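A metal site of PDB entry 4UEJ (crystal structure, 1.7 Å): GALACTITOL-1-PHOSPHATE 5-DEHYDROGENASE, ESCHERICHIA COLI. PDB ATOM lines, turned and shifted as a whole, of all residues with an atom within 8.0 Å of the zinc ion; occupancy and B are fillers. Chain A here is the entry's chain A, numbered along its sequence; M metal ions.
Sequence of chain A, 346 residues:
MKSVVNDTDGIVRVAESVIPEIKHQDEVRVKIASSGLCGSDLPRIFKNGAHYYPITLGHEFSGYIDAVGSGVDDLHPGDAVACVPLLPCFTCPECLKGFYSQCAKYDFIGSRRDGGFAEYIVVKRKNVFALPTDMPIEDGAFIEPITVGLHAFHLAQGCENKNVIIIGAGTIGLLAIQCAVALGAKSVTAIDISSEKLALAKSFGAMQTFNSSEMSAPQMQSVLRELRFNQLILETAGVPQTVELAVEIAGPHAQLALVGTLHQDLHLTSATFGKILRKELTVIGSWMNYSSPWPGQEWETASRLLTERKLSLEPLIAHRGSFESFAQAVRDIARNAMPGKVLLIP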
ATOM      1  N   LEU A  87     -21.013  -6.916  17.747  1.00  0.00           N
ATOM      2  CA  LEU A  87     -21.153  -5.467  17.856  1.00  0.00           C
ATOM      3  C   LEU A  87     -22.461  -5.052  17.196  1.00  0.00           C
ATOM      4  O   LEU A  87     -22.529  -4.889  15.986  1.00  0.00           O
ATOM      5  CB  LEU A  87     -19.970  -4.740  17.215  1.00  0.00           C
ATOM      6  CG  LEU A  87     -19.960  -3.222  17.427  1.00  0.00           C
ATOM      7  CD1 LEU A  87     -19.721  -2.866  18.894  1.00  0.00           C
ATOM      8  CD2 LEU A  87     -18.932  -2.525  16.524  1.00  0.00           C
ATOM      9  N   PRO A  88     -23.509  -4.886  18.017  1.00  0.00           N
ATOM     10  CA  PRO A  88     -24.763  -4.352  17.475  1.00  0.00           C
ATOM     11  C   PRO A  88     -24.613  -2.868  17.138  1.00  0.00           C
ATOM     12  O   PRO A  88     -23.646  -2.222  17.572  1.00  0.00           O
ATOM     13  CB  PRO A  88     -25.770  -4.564  18.607  1.00  0.00           C
ATOM     14  CG  PRO A  88     -24.974  -4.740  19.837  1.00  0.00           C
ATOM     15  CD  PRO A  88     -23.590  -5.166  19.458  1.00  0.00           C
ATOM     16  N   CYS A  89     -25.564  -2.337  16.383  1.00  0.00           N
ATOM     17  CA  CYS A  89     -25.520  -0.929  15.970  1.00  0.00           C
ATOM     18  C   CYS A  89     -26.022  -0.012  17.091  1.00  0.00           C
ATOM     19  O   CYS A  89     -25.647   1.177  17.142  1.00  0.00           O
ATOM     20  CB  CYS A  89     -26.340  -0.704  14.692  1.00  0.00           C
ATOM     21  SG  CYS A  89     -28.138  -0.530  14.922  1.00  0.00           S
ATOM     22  N   PHE A  90     -26.849  -0.576  17.971  1.00  0.00           N
ATOM     23  CA  PHE A  90     -27.419   0.088  19.151  1.00  0.00           C
ATOM     24  C   PHE A  90     -28.414   1.202  18.850  1.00  0.00           C
ATOM     25  O   PHE A  90     -28.813   1.936  19.761  1.00  0.00           O
ATOM     26  CB  PHE A  90     -26.304   0.651  20.050  1.00  0.00           C
ATOM     27  CG  PHE A  90     -25.495  -0.396  20.722  1.00  0.00           C
ATOM     28  CD1 PHE A  90     -26.065  -1.227  21.667  1.00  0.00           C
ATOM     29  CD2 PHE A  90     -24.146  -0.528  20.439  1.00  0.00           C
ATOM     30  CE1 PHE A  90     -25.310  -2.198  22.302  1.00  0.00           C
ATOM     31  CE2 PHE A  90     -23.384  -1.496  21.062  1.00  0.00           C
ATOM     32  CZ  PHE A  90     -23.969  -2.320  21.997  1.00  0.00           C
ATOM     33  N   THR A  91     -28.815   1.336  17.588  1.00  0.00           N
ATOM     34  CA  THR A  91     -29.702   2.450  17.228  1.00  0.00           C
ATOM     35  C   THR A  91     -30.901   2.049  16.375  1.00  0.00           C
ATOM     36  O   THR A  91     -31.726   2.892  16.046  1.00  0.00           O
ATOM     37  CB  THR A  91     -28.936   3.558  16.484  1.00  0.00           C
ATOM     38  OG1 THR A  91     -28.452   3.045  15.235  1.00  0.00           O
ATOM     39  CG2 THR A  91     -27.764   4.065  17.323  1.00  0.00           C
ATOM     40  N   CYS A  92     -31.000   0.774  15.999  1.00  0.00           N
ATOM     41  CA  CYS A  92     -32.164   0.297  15.239  1.00  0.00           C
ATOM     42  C   CYS A  92     -33.252  -0.119  16.226  1.00  0.00           C
ATOM     43  O   CYS A  92     -32.974  -0.267  17.406  1.00  0.00           O
ATOM     44  CB  CYS A  92     -31.787  -0.880  14.337  1.00  0.00           C
ATOM     45  SG  CYS A  92     -31.373  -2.385  15.251  1.00  0.00           S
ATOM     46  N   PRO A  93     -34.499  -0.290  15.747  1.00  0.00           N
ATOM     47  CA  PRO A  93     -35.576  -0.648  16.677  1.00  0.00           C
ATOM     48  C   PRO A  93     -35.323  -1.924  17.454  1.00  0.00           C
ATOM     49  O   PRO A  93     -35.641  -1.958  18.644  1.00  0.00           O
ATOM     50  CB  PRO A  93     -36.788  -0.812  15.742  1.00  0.00           C
ATOM     51  CG  PRO A  93     -36.498   0.104  14.614  1.00  0.00           C
ATOM     52  CD  PRO A  93     -35.008   0.002  14.394  1.00  0.00           C
ATOM     53  N   GLU A  94     -34.765  -2.944  16.813  1.00  0.00           N
ATOM     54  CA  GLU A  94     -34.426  -4.190  17.507  1.00  0.00           C
ATOM     55  C   GLU A  94     -33.448  -3.926  18.660  1.00  0.00           C
ATOM     56  O   GLU A  94     -33.665  -4.398  19.777  1.00  0.00           O
ATOM     57  CB  GLU A  94     -33.843  -5.208  16.531  1.00  0.00           C
ATOM     58  CG  GLU A  94     -34.872  -5.970  15.683  1.00  0.00           C
ATOM     59  CD  GLU A  94     -35.354  -5.188  14.461  1.00  0.00           C
ATOM     60  OE1 GLU A  94     -35.037  -3.982  14.342  1.00  0.00           O
ATOM     61  OE2 GLU A  94     -36.051  -5.795  13.621  1.00  0.00           O
ATOM     62  N   CYS A  95     -32.388  -3.174  18.396  1.00  0.00           N
ATOM     63  CA  CYS A  95     -31.393  -2.886  19.427  1.00  0.00           C
ATOM     64  C   CYS A  95     -32.015  -2.104  20.580  1.00  0.00           C
ATOM     65  O   CYS A  95     -31.738  -2.377  21.742  1.00  0.00           O
ATOM     66  CB  CYS A  95     -30.203  -2.099  18.871  1.00  0.00           C
ATOM     67  SG  CYS A  95     -28.979  -3.065  17.973  1.00  0.00           S
ATOM     68  N   LEU A  96     -32.873  -1.138  20.261  1.00  0.00           N
ATOM     69  CA  LEU A  96     -33.499  -0.336  21.303  1.00  0.00           C
ATOM     70  C   LEU A  96     -34.451  -1.167  22.153  1.00  0.00           C
ATOM     71  O   LEU A  96     -34.815  -0.757  23.255  1.00  0.00           O
ATOM     72  CB  LEU A  96     -34.228   0.862  20.688  1.00  0.00           C
ATOM     73  CG  LEU A  96     -33.314   1.854  19.957  1.00  0.00           C
ATOM     74  CD1 LEU A  96     -34.138   2.932  19.273  1.00  0.00           C
ATOM     75  CD2 LEU A  96     -32.285   2.482  20.890  1.00  0.00           C
ATOM     76  N   PHE A  99     -33.017  -6.456  21.574  1.00  0.00           N
ATOM     77  CA  PHE A  99     -32.916  -7.588  20.672  1.00  0.00           C
ATOM     78  C   PHE A  99     -31.636  -7.494  19.840  1.00  0.00           C
ATOM     79  O   PHE A  99     -31.697  -7.353  18.621  1.00  0.00           O
ATOM     80  CB  PHE A  99     -34.130  -7.639  19.749  1.00  0.00           C
ATOM     81  CG  PHE A  99     -35.441  -7.781  20.483  1.00  0.00           C
ATOM     82  CD1 PHE A  99     -35.490  -8.270  21.775  1.00  0.00           C
ATOM     83  CD2 PHE A  99     -36.628  -7.442  19.852  1.00  0.00           C
ATOM     84  CE1 PHE A  99     -36.686  -8.410  22.439  1.00  0.00           C
ATOM     85  CE2 PHE A  99     -37.832  -7.577  20.512  1.00  0.00           C
ATOM     86  CZ  PHE A  99     -37.868  -8.063  21.805  1.00  0.00           C
ATOM     87  N   TYR A 100     -30.489  -7.606  20.498  1.00  0.00           N
ATOM     88  CA  TYR A 100     -29.212  -7.283  19.846  1.00  0.00           C
ATOM     89  C   TYR A 100     -28.854  -8.282  18.779  1.00  0.00           C
ATOM     90  O   TYR A 100     -28.250  -7.936  17.752  1.00  0.00           O
ATOM     91  CB  TYR A 100     -28.093  -7.206  20.874  1.00  0.00           C
ATOM     92  CG  TYR A 100     -28.359  -6.201  21.961  1.00  0.00           C
ATOM     93  CD1 TYR A 100     -28.376  -4.848  21.677  1.00  0.00           C
ATOM     94  CD2 TYR A 100     -28.564  -6.607  23.270  1.00  0.00           C
ATOM     95  CE1 TYR A 100     -28.623  -3.913  22.668  1.00  0.00           C
ATOM     96  CE2 TYR A 100     -28.800  -5.687  24.273  1.00  0.00           C
ATOM     97  CZ  TYR A 100     -28.830  -4.337  23.964  1.00  0.00           C
ATOM     98  OH  TYR A 100     -29.072  -3.419  24.954  1.00  0.00           O
ATOM     99  N   SER A 101     -29.221  -9.529  19.020  1.00  0.00           N
ATOM    100  CA  SER A 101     -28.910 -10.585  18.099  1.00  0.00           C
ATOM    101  C   SER A 101     -29.811 -10.569  16.872  1.00  0.00           C
ATOM    102  O   SER A 101     -29.599 -11.329  15.919  1.00  0.00           O
ATOM    103  CB  SER A 101     -28.985 -11.937  18.818  1.00  0.00           C
ATOM    104  OG  SER A 101     -28.088 -11.904  19.916  1.00  0.00           O
ATOM    105  N   GLN A 102     -30.800  -9.669  16.866  1.00  0.00           N
ATOM    106  CA  GLN A 102     -31.613  -9.445  15.686  1.00  0.00           C
ATOM    107  C   GLN A 102     -31.270  -8.118  15.000  1.00  0.00           C
ATOM    108  O   GLN A 102     -31.982  -7.668  14.102  1.00  0.00           O
ATOM    109  CB  GLN A 102     -33.110  -9.467  16.032  1.00  0.00           C
ATOM    110  CG  GLN A 102     -33.641 -10.885  16.329  1.00  0.00           C
ATOM    111  CD  GLN A 102     -33.276 -11.360  17.715  1.00  0.00           C
ATOM    112  OE1 GLN A 102     -33.429 -10.633  18.691  1.00  0.00           O
ATOM    113  NE2 GLN A 102     -32.776 -12.597  17.814  1.00  0.00           N
ATOM    114  N   CYS A 103     -30.178  -7.497  15.433  1.00  0.00           N
ATOM    115  CA  CYS A 103     -29.712  -6.298  14.750  1.00  0.00           C
ATOM    116  C   CYS A 103     -29.415  -6.653  13.281  1.00  0.00           C
ATOM    117  O   CYS A 103     -28.782  -7.679  13.013  1.00  0.00           O
ATOM    118  CB  CYS A 103     -28.470  -5.732  15.424  1.00  0.00           C
ATOM    119  SG  CYS A 103     -27.817  -4.288  14.595  1.00  0.00           S
ATOM    120  N   ALA A 104     -29.897  -5.848  12.347  1.00  0.00           N
ATOM    121  CA  ALA A 104     -29.691  -6.151  10.932  1.00  0.00           C
ATOM    122  C   ALA A 104     -28.280  -5.761  10.502  1.00  0.00           C
ATOM    123  O   ALA A 104     -27.745  -6.296   9.521  1.00  0.00           O
ATOM    124  CB  ALA A 104     -30.723  -5.448  10.072  1.00  0.00           C
ATOM    125  N   LYS A 105     -27.675  -4.837  11.250  1.00  0.00           N
ATOM    126  CA  LYS A 105     -26.350  -4.340  10.912  1.00  0.00           C
ATOM    127  C   LYS A 105     -25.357  -4.563  12.038  1.00  0.00           C
ATOM    128  O   LYS A 105     -24.772  -3.609  12.557  1.00  0.00           O
ATOM    129  CB  LYS A 105     -26.423  -2.852  10.577  1.00  0.00           C
ATOM    130  CG  LYS A 105     -25.571  -2.429   9.393  1.00  0.00           C
ATOM    131  CD  LYS A 105     -25.178  -0.961   9.477  1.00  0.00           C
ATOM    132  CE  LYS A 105     -25.215  -0.314   8.100  1.00  0.00           C
ATOM    133  NZ  LYS A 105     -24.344   0.892   8.033  1.00  0.00           N
ATOM    134  N   TYR A 106     -25.148  -5.813  12.425  1.00  0.00           N
ATOM    135  CA  TYR A 106     -24.185  -6.096  13.485  1.00  0.00           C
ATOM    136  C   TYR A 106     -22.882  -6.629  12.912  1.00  0.00           C
ATOM    137  O   TYR A 106     -22.862  -7.278  11.865  1.00  0.00           O
ATOM    138  CB  TYR A 106     -24.761  -7.045  14.539  1.00  0.00           C
ATOM    139  CG  TYR A 106     -25.032  -8.498  14.161  1.00  0.00           C
ATOM    140  CD1 TYR A 106     -23.987  -9.415  13.986  1.00  0.00           C
ATOM    141  CD2 TYR A 106     -26.327  -8.977  14.060  1.00  0.00           C
ATOM    142  CE1 TYR A 106     -24.238 -10.750  13.695  1.00  0.00           C
ATOM    143  CE2 TYR A 106     -26.587 -10.302  13.749  1.00  0.00           C
ATOM    144  CZ  TYR A 106     -25.545 -11.178  13.571  1.00  0.00           C
ATOM    145  OH  TYR A 106     -25.812 -12.506  13.271  1.00  0.00           O
HETATM  146 ZN    ZN M   1     -29.098  -2.517  15.718  1.00  0.00          ZN
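N of Phe 90 sits close to SG of Cys 95 (3.3 Å).
The backbone NH (N) of Glu 94 sits close to the side-chain sulfur (SG) of Cys 92 (3.8 Å).
SG of Cys 89 lies close to N of Thr 91, 3.3 Å away.
The side-chain sulfur (SG) of Cys 103 lies close to the backbone NH (N) of Lys 105, at 3.4 Å.
SG of Cys 103 lies close to N of Tyr 106, at 3.8 Å.
The zinc ion is bound by the side-chain sulfur of Cys 95 (2.3 Å), the side-chain sulfur of Cys 92 (2.3 Å), the side-chain sulfur of Cys 89 (2.3 Å) and the side-chain sulfur of Cys 103 (2.5 Å).
Residues that only touch the zinc ion: Phe 90 (3.7 Å).
The nearest printed residue that does not touch the zinc ion is Thr 91 (4.3 Å).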
